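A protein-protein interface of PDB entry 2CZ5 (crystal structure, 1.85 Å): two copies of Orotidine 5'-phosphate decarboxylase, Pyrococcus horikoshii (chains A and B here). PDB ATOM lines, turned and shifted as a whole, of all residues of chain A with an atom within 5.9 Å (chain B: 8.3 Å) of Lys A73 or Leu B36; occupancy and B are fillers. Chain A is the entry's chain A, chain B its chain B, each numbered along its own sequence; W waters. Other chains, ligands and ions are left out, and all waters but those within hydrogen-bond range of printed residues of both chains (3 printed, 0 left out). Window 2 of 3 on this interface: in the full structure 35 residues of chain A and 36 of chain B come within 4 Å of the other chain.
Trp A32 touches Trp B32.
Leu B36 touches Trp A32.
CD2 of Leu B36 touches CG2 of Ile A35 (3.6 Å).
Leu B36 touches Val A40 (CD2 to CB, 3.9 Å).
Leu A69 touches Tyr B9 (CD1 to OH, 3.6 Å).
CG of Pro B33 touches CB of Leu A69, 3.7 Å away.
Ile A70 touches Trp B32 (CD1 to CB, 3.7 Å).
CG1 of Ile A70 touches CD of Pro B33, at 3.6 Å.
Lys A73 touches Leu B36.
Water W3 bridges O of Leu B36 (2.7 Å) and N of Val A40 (3.1 Å).
Water W2 lies within hydrogen-bond range of the backbone carbonyl oxygen of Leu B36 (3.1 Å), the side-chain amino group of Lys A73 (3.1 Å) and the backbone carbonyl oxygen of Gly B37 (3.5 Å).
Water W1 bridges the backbone carbonyl oxygen (O) of Ile B35 (3.2 Å) and the backbone carbonyl oxygen (O) of Ile A35 (3.3 Å).
Of the 12 printed residues of chain B, 4 touch a printed residue of chain A.
Printed residues of chain B that touch a printed residue of chain A: Tyr B9, Trp B32, Pro B33 and Leu B36.
Along chain B the printed residues that touch a printed residue of chain A span positions 9 to 36.
Of the 14 printed residues of chain A, 6 touch a printed residue of chain B.
Printed residues of chain A that touch a printed residue of chain B: Trp A32, Ile A35, Val A40, Leu A69, Ile A70 and Lys A73.
Among the printed residues, no Asp or Glu carboxylate lies within 4 Å of a Lys or Arg side-chain nitrogen of the other chain.
The side-chain hydroxyl (OH) of Tyr B9 is in hydrogen-bond range of the side-chain amide nitrogen (ND2) of Asn B31 (3.0 Å).
Of the printed residues of chain B, Lys A73 touches Leu B36.
Leu B36 touches just these residues of chain A: Trp A32 (3.9 Å), Ile A35 (3.6 Å), Val A40 (3.9 Å) and Lys A73 (3.9 Å).
Printed residues of chain B within 4 Å of Trp A32: Trp B32 (3.4 Å) and Leu B36 (3.9 Å).
Printed residues of chain B within 4 Å of Leu A69: Tyr B9 and Pro B33.
Printed residues of chain A within 4 Å of Tyr B9: Leu A69.
The nearest residue of chain A that does not touch Leu B36 is Ile A70 (4.03 Å).
The nearest printed residue of chain A that does not touch Pro B33 is Lys A73 (5.7 Å).
Trp A32 touches its own counterpart, Trp B32.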
ATOM      1  N   TRP A  32      11.930   0.630   0.155  1.00  0.00           N
ATOM      2  CA  TRP A  32      12.891   0.540  -0.936  1.00  0.00           C
ATOM      3  C   TRP A  32      12.286   0.215  -2.315  1.00  0.00           C
ATOM      4  O   TRP A  32      12.818   0.647  -3.331  1.00  0.00           O
ATOM      5  CB  TRP A  32      14.005  -0.464  -0.578  1.00  0.00           C
ATOM      6  CG  TRP A  32      14.858  -0.058   0.628  1.00  0.00           C
ATOM      7  CD1 TRP A  32      14.950  -0.720   1.817  1.00  0.00           C
ATOM      8  CD2 TRP A  32      15.770   1.051   0.718  1.00  0.00           C
ATOM      9  NE1 TRP A  32      15.864  -0.100   2.640  1.00  0.00           N
ATOM     10  CE2 TRP A  32      16.380   0.990   1.991  1.00  0.00           C
ATOM     11  CE3 TRP A  32      16.128   2.092  -0.156  1.00  0.00           C
ATOM     12  CZ2 TRP A  32      17.329   1.927   2.417  1.00  0.00           C
ATOM     13  CZ3 TRP A  32      17.078   3.029   0.267  1.00  0.00           C
ATOM     14  CH2 TRP A  32      17.664   2.937   1.547  1.00  0.00           C
ATOM     15  N   ILE A  35      11.376   3.587  -3.836  1.00  0.00           N
ATOM     16  CA  ILE A  35      12.528   4.457  -4.008  1.00  0.00           C
ATOM     17  C   ILE A  35      13.367   3.920  -5.182  1.00  0.00           C
ATOM     18  O   ILE A  35      13.884   4.691  -5.983  1.00  0.00           O
ATOM     19  CB  ILE A  35      13.373   4.535  -2.736  1.00  0.00           C
ATOM     20  CG1 ILE A  35      12.652   5.419  -1.702  1.00  0.00           C
ATOM     21  CG2 ILE A  35      14.771   5.104  -3.066  1.00  0.00           C
ATOM     22  CD1 ILE A  35      13.200   5.294  -0.281  1.00  0.00           C
ATOM     23  N   VAL A  40      14.659   8.434  -5.237  1.00  0.00           N
ATOM     24  CA  VAL A  40      14.355   8.922  -3.895  1.00  0.00           C
ATOM     25  C   VAL A  40      13.557  10.223  -3.909  1.00  0.00           C
ATOM     26  O   VAL A  40      12.966  10.609  -2.897  1.00  0.00           O
ATOM     27  CB  VAL A  40      15.648   9.129  -3.079  1.00  0.00           C
ATOM     28  CG1 VAL A  40      16.474  10.258  -3.677  1.00  0.00           C
ATOM     29  CG2 VAL A  40      15.303   9.411  -1.619  1.00  0.00           C
ATOM     30  N   ARG A  68      24.017   6.900   8.883  1.00  0.00           N
ATOM     31  CA  ARG A  68      24.017   8.368   8.850  1.00  0.00           C
ATOM     32  C   ARG A  68      23.928   8.889   7.429  1.00  0.00           C
ATOM     33  O   ARG A  68      23.136   9.789   7.132  1.00  0.00           O
ATOM     34  CB  ARG A  68      25.284   8.913   9.520  1.00  0.00           C
ATOM     35  CG  ARG A  68      25.386  10.418   9.573  1.00  0.00           C
ATOM     36  CD  ARG A  68      26.622  10.852  10.379  1.00  0.00           C
ATOM     37  NE  ARG A  68      26.646  10.277  11.727  1.00  0.00           N
ATOM     38  CZ  ARG A  68      27.484   9.321  12.128  1.00  0.00           C
ATOM     39  NH1 ARG A  68      28.380   8.822  11.287  1.00  0.00           N
ATOM     40  NH2 ARG A  68      27.430   8.864  13.376  1.00  0.00           N
ATOM     41  N   LEU A  69      24.736   8.319   6.542  1.00  0.00           N
ATOM     42  CA  LEU A  69      24.729   8.743   5.148  1.00  0.00           C
ATOM     43  C   LEU A  69      23.348   8.520   4.529  1.00  0.00           C
ATOM     44  O   LEU A  69      22.843   9.373   3.795  1.00  0.00           O
ATOM     45  CB  LEU A  69      25.786   7.978   4.344  1.00  0.00           C
ATOM     46  CG  LEU A  69      27.261   8.344   4.559  1.00  0.00           C
ATOM     47  CD1 LEU A  69      28.142   7.491   3.658  1.00  0.00           C
ATOM     48  CD2 LEU A  69      27.468   9.824   4.258  1.00  0.00           C
ATOM     49  N   ILE A  70      22.738   7.373   4.821  1.00  0.00           N
ATOM     50  CA  ILE A  70      21.419   7.070   4.278  1.00  0.00           C
ATOM     51  C   ILE A  70      20.375   8.005   4.897  1.00  0.00           C
ATOM     52  O   ILE A  70      19.552   8.599   4.201  1.00  0.00           O
ATOM     53  CB  ILE A  70      21.018   5.586   4.550  1.00  0.00           C
ATOM     54  CG1 ILE A  70      21.969   4.630   3.802  1.00  0.00           C
ATOM     55  CG2 ILE A  70      19.559   5.341   4.084  1.00  0.00           C
ATOM     56  CD1 ILE A  70      21.952   3.203   4.352  1.00  0.00           C
ATOM     57  N   ALA A  71      20.413   8.154   6.213  1.00  0.00           N
ATOM     58  CA  ALA A  71      19.434   9.030   6.853  1.00  0.00           C
ATOM     59  C   ALA A  71      19.537  10.449   6.312  1.00  0.00           C
ATOM     60  O   ALA A  71      18.534  11.054   5.942  1.00  0.00           O
ATOM     61  CB  ALA A  71      19.631   9.029   8.361  1.00  0.00           C
ATOM     62  N   ARG A  72      20.747  10.995   6.275  1.00  0.00           N
ATOM     63  CA  ARG A  72      20.943  12.352   5.780  1.00  0.00           C
ATOM     64  C   ARG A  72      20.351  12.518   4.386  1.00  0.00           C
ATOM     65  O   ARG A  72      19.702  13.516   4.089  1.00  0.00           O
ATOM     66  CB  ARG A  72      22.432  12.707   5.746  1.00  0.00           C
ATOM     67  CG  ARG A  72      22.701  14.146   6.151  1.00  0.00           C
ATOM     68  CD  ARG A  72      23.741  14.793   5.268  1.00  0.00           C
ATOM     69  NE  ARG A  72      24.887  13.924   5.032  1.00  0.00           N
ATOM     70  CZ  ARG A  72      25.791  14.139   4.080  1.00  0.00           C
ATOM     71  NH1 ARG A  72      25.674  15.201   3.287  1.00  0.00           N
ATOM     72  NH2 ARG A  72      26.797  13.290   3.906  1.00  0.00           N
ATOM     73  N   LYS A  73      20.580  11.539   3.518  1.00  0.00           N
ATOM     74  CA  LYS A  73      20.038  11.609   2.165  1.00  0.00           C
ATOM     75  C   LYS A  73      18.509  11.546   2.125  1.00  0.00           C
ATOM     76  O   LYS A  73      17.852  12.339   1.433  1.00  0.00           O
ATOM     77  CB  LYS A  73      20.610  10.468   1.317  1.00  0.00           C
ATOM     78  CG  LYS A  73      20.036  10.425  -0.101  1.00  0.00           C
ATOM     79  CD  LYS A  73      20.492  11.631  -0.930  1.00  0.00           C
ATOM     80  CE  LYS A  73      20.233  11.411  -2.418  1.00  0.00           C
ATOM     81  NZ  LYS A  73      20.819  12.492  -3.269  1.00  0.00           N
ATOM     82  N   VAL A  74      17.936  10.605   2.867  1.00  0.00           N
ATOM     83  CA  VAL A  74      16.490  10.435   2.863  1.00  0.00           C
ATOM     84  C   VAL A  74      15.720  11.544   3.580  1.00  0.00           C
ATOM     85  O   VAL A  74      14.676  12.000   3.083  1.00  0.00           O
ATOM     86  CB  VAL A  74      16.141   9.040   3.390  1.00  0.00           C
ATOM     87  CG1 VAL A  74      14.646   8.877   3.531  1.00  0.00           C
ATOM     88  CG2 VAL A  74      16.670   8.007   2.388  1.00  0.00           C
ATOM     89  N   PHE A  75      16.239  11.995   4.721  1.00  0.00           N
ATOM     90  CA  PHE A  75      15.607  13.106   5.439  1.00  0.00           C
ATOM     91  C   PHE A  75      15.757  14.348   4.541  1.00  0.00           C
ATOM     92  O   PHE A  75      14.838  15.146   4.393  1.00  0.00           O
ATOM     93  CB  PHE A  75      16.305  13.366   6.780  1.00  0.00           C
ATOM     94  CG  PHE A  75      15.879  12.433   7.897  1.00  0.00           C
ATOM     95  CD1 PHE A  75      14.532  12.270   8.213  1.00  0.00           C
ATOM     96  CD2 PHE A  75      16.825  11.751   8.651  1.00  0.00           C
ATOM     97  CE1 PHE A  75      14.127  11.433   9.273  1.00  0.00           C
ATOM     98  CE2 PHE A  75      16.443  10.914   9.708  1.00  0.00           C
ATOM     99  CZ  PHE A  75      15.084  10.754  10.019  1.00  0.00           C
ATOM    100  N   GLY A  76      16.925  14.493   3.926  1.00  0.00           N
ATOM    101  CA  GLY A  76      17.150  15.631   3.049  1.00  0.00           C
ATOM    102  C   GLY A  76      16.255  15.634   1.820  1.00  0.00           C
ATOM    103  O   GLY A  76      16.057  16.674   1.186  1.00  0.00           O
ATOM    104  N   ALA A  77      15.701  14.471   1.488  1.00  0.00           N
ATOM    105  CA  ALA A  77      14.820  14.338   0.335  1.00  0.00           C
ATOM    106  C   ALA A  77      13.372  14.565   0.750  1.00  0.00           C
ATOM    107  O   ALA A  77      12.456  14.405  -0.049  1.00  0.00           O
ATOM    108  CB  ALA A  77      14.984  12.944  -0.297  1.00  0.00           C
ATOM    109  N   GLY A  78      13.168  14.930   2.011  1.00  0.00           N
ATOM    110  CA  GLY A  78      11.820  15.182   2.487  1.00  0.00           C
ATOM    111  C   GLY A  78      11.166  14.173   3.426  1.00  0.00           C
ATOM    112  O   GLY A  78      10.005  14.357   3.792  1.00  0.00           O
ATOM    113  N   TYR B   9      30.520   8.866  -3.821  1.00  0.00           N
ATOM    114  CA  TYR B   9      29.176   9.264  -4.206  1.00  0.00           C
ATOM    115  C   TYR B   9      28.991  10.251  -5.356  1.00  0.00           C
ATOM    116  O   TYR B   9      27.871  10.631  -5.691  1.00  0.00           O
ATOM    117  CB  TYR B   9      28.441   9.676  -2.919  1.00  0.00           C
ATOM    118  CG  TYR B   9      28.643   8.605  -1.847  1.00  0.00           C
ATOM    119  CD1 TYR B   9      28.253   7.287  -2.085  1.00  0.00           C
ATOM    120  CD2 TYR B   9      29.280   8.890  -0.637  1.00  0.00           C
ATOM    121  CE1 TYR B   9      28.493   6.278  -1.164  1.00  0.00           C
ATOM    122  CE2 TYR B   9      29.527   7.870   0.308  1.00  0.00           C
ATOM    123  CZ  TYR B   9      29.128   6.565   0.028  1.00  0.00           C
ATOM    124  OH  TYR B   9      29.366   5.528   0.911  1.00  0.00           O
ATOM    125  N   ASN B  31      26.691   0.500  -2.038  1.00  0.00           N
ATOM    126  CA  ASN B  31      25.791   0.562  -0.893  1.00  0.00           C
ATOM    127  C   ASN B  31      24.516   1.372  -1.171  1.00  0.00           C
ATOM    128  O   ASN B  31      24.310   1.849  -2.283  1.00  0.00           O
ATOM    129  CB  ASN B  31      26.511   1.137   0.340  1.00  0.00           C
ATOM    130  CG  ASN B  31      27.121   2.514   0.107  1.00  0.00           C
ATOM    131  OD1 ASN B  31      26.760   3.243  -0.826  1.00  0.00           O
ATOM    132  ND2 ASN B  31      28.025   2.894   0.995  1.00  0.00           N
ATOM    133  N   TRP B  32      23.670   1.552  -0.156  1.00  0.00           N
ATOM    134  CA  TRP B  32      22.452   2.322  -0.375  1.00  0.00           C
ATOM    135  C   TRP B  32      22.781   3.784  -0.724  1.00  0.00           C
ATOM    136  O   TRP B  32      22.137   4.369  -1.583  1.00  0.00           O
ATOM    137  CB  TRP B  32      21.520   2.251   0.836  1.00  0.00           C
ATOM    138  CG  TRP B  32      20.628   1.012   0.909  1.00  0.00           C
ATOM    139  CD1 TRP B  32      20.506   0.155   1.968  1.00  0.00           C
ATOM    140  CD2 TRP B  32      19.690   0.554  -0.079  1.00  0.00           C
ATOM    141  NE1 TRP B  32      19.550  -0.800   1.706  1.00  0.00           N
ATOM    142  CE2 TRP B  32      19.034  -0.582   0.458  1.00  0.00           C
ATOM    143  CE3 TRP B  32      19.340   0.990  -1.369  1.00  0.00           C
ATOM    144  CZ2 TRP B  32      18.048  -1.291  -0.247  1.00  0.00           C
ATOM    145  CZ3 TRP B  32      18.357   0.282  -2.070  1.00  0.00           C
ATOM    146  CH2 TRP B  32      17.726  -0.845  -1.503  1.00  0.00           C
ATOM    147  N   PRO B  33      23.775   4.398  -0.050  1.00  0.00           N
ATOM    148  CA  PRO B  33      24.068   5.794  -0.412  1.00  0.00           C
ATOM    149  C   PRO B  33      24.348   6.012  -1.917  1.00  0.00           C
ATOM    150  O   PRO B  33      23.858   6.971  -2.514  1.00  0.00           O
ATOM    151  CB  PRO B  33      25.256   6.129   0.476  1.00  0.00           C
ATOM    152  CG  PRO B  33      24.877   5.411   1.769  1.00  0.00           C
ATOM    153  CD  PRO B  33      24.392   4.050   1.247  1.00  0.00           C
ATOM    154  N   LEU B  34      25.122   5.128  -2.531  1.00  0.00           N
ATOM    155  CA  LEU B  34      25.414   5.273  -3.958  1.00  0.00           C
ATOM    156  C   LEU B  34      24.140   5.061  -4.784  1.00  0.00           C
ATOM    157  O   LEU B  34      23.848   5.844  -5.687  1.00  0.00           O
ATOM    158  CB  LEU B  34      26.510   4.284  -4.388  1.00  0.00           C
ATOM    159  CG  LEU B  34      26.900   4.280  -5.876  1.00  0.00           C
ATOM    160  CD1 LEU B  34      27.217   5.706  -6.369  1.00  0.00           C
ATOM    161  CD2 LEU B  34      28.099   3.368  -6.065  1.00  0.00           C
ATOM    162  N   ILE B  35      23.383   4.007  -4.481  1.00  0.00           N
ATOM    163  CA  ILE B  35      22.137   3.725  -5.203  1.00  0.00           C
ATOM    164  C   ILE B  35      21.141   4.885  -5.059  1.00  0.00           C
ATOM    165  O   ILE B  35      20.404   5.206  -5.985  1.00  0.00           O
ATOM    166  CB  ILE B  35      21.475   2.407  -4.695  1.00  0.00           C
ATOM    167  CG1 ILE B  35      22.350   1.205  -5.100  1.00  0.00           C
ATOM    168  CG2 ILE B  35      20.042   2.274  -5.270  1.00  0.00           C
ATOM    169  CD1 ILE B  35      22.014  -0.107  -4.376  1.00  0.00           C
ATOM    170  N   LEU B  36      21.115   5.516  -3.886  1.00  0.00           N
ATOM    171  CA  LEU B  36      20.215   6.632  -3.672  1.00  0.00           C
ATOM    172  C   LEU B  36      20.636   7.839  -4.496  1.00  0.00           C
ATOM    173  O   LEU B  36      19.796   8.526  -5.070  1.00  0.00           O
ATOM    174  CB  LEU B  36      20.194   7.019  -2.177  1.00  0.00           C
ATOM    175  CG  LEU B  36      19.351   6.087  -1.308  1.00  0.00           C
ATOM    176  CD1 LEU B  36      19.673   6.325   0.179  1.00  0.00           C
ATOM    177  CD2 LEU B  36      17.873   6.342  -1.608  1.00  0.00           C
ATOM    178  N   GLY B  37      21.937   8.089  -4.578  1.00  0.00           N
ATOM    179  CA  GLY B  37      22.396   9.246  -5.329  1.00  0.00           C
ATOM    180  C   GLY B  37      22.429   9.093  -6.840  1.00  0.00           C
ATOM    181  O   GLY B  37      22.119  10.031  -7.572  1.00  0.00           O
ATOM    182  N   SER B  38      22.797   7.908  -7.311  1.00  0.00           N
ATOM    183  CA  SER B  38      22.905   7.656  -8.749  1.00  0.00           C
ATOM    184  C   SER B  38      21.741   6.874  -9.345  1.00  0.00           C
ATOM    185  O   SER B  38      21.600   6.793 -10.578  1.00  0.00           O
ATOM    186  CB  SER B  38      24.210   6.900  -9.037  1.00  0.00           C
ATOM    187  OG  SER B  38      25.364   7.695  -8.764  1.00  0.00           O
ATOM    188  N   GLY B  39      20.908   6.291  -8.487  1.00  0.00           N
ATOM    189  CA  GLY B  39      19.804   5.495  -8.988  1.00  0.00           C
ATOM    190  C   GLY B  39      20.254   4.043  -9.119  1.00  0.00           C
ATOM    191  O   GLY B  39      21.453   3.760  -9.212  1.00  0.00           O
ATOM    192  N   VAL B  40      19.303   3.118  -9.126  1.00  0.00           N
ATOM    193  CA  VAL B  40      19.633   1.713  -9.230  1.00  0.00           C
ATOM    194  C   VAL B  40      20.293   1.355 -10.580  1.00  0.00           C
ATOM    195  O   VAL B  40      20.902   0.295 -10.726  1.00  0.00           O
ATOM    196  CB  VAL B  40      18.378   0.847  -8.984  1.00  0.00           C
ATOM    197  CG1 VAL B  40      17.374   1.036 -10.104  1.00  0.00           C
ATOM    198  CG2 VAL B  40      18.781  -0.612  -8.829  1.00  0.00           C
ATOM    199  N   ILE B  42      22.871   2.540 -11.634  1.00  0.00           N
ATOM    200  CA  ILE B  42      24.323   2.639 -11.447  1.00  0.00           C
ATOM    201  C   ILE B  42      24.926   1.219 -11.501  1.00  0.00           C
ATOM    202  O   ILE B  42      26.083   1.038 -11.857  1.00  0.00           O
ATOM    203  CB  ILE B  42      24.682   3.258 -10.067  1.00  0.00           C
ATOM    204  CG1 ILE B  42      26.182   3.520  -9.980  1.00  0.00           C
ATOM    205  CG2 ILE B  42      24.307   2.304  -8.953  1.00  0.00           C
ATOM    206  CD1 ILE B  42      26.626   4.686 -10.822  1.00  0.00           C
HETATM  207  O   HOH W   1      17.185   4.821  -6.040  1.00  0.00           O
HETATM  208  O   HOH W   2      19.440  11.509  -5.913  1.00  0.00           O
HETATM  209  O   HOH W   3      17.470   7.508  -6.096  1.00  0.00           O
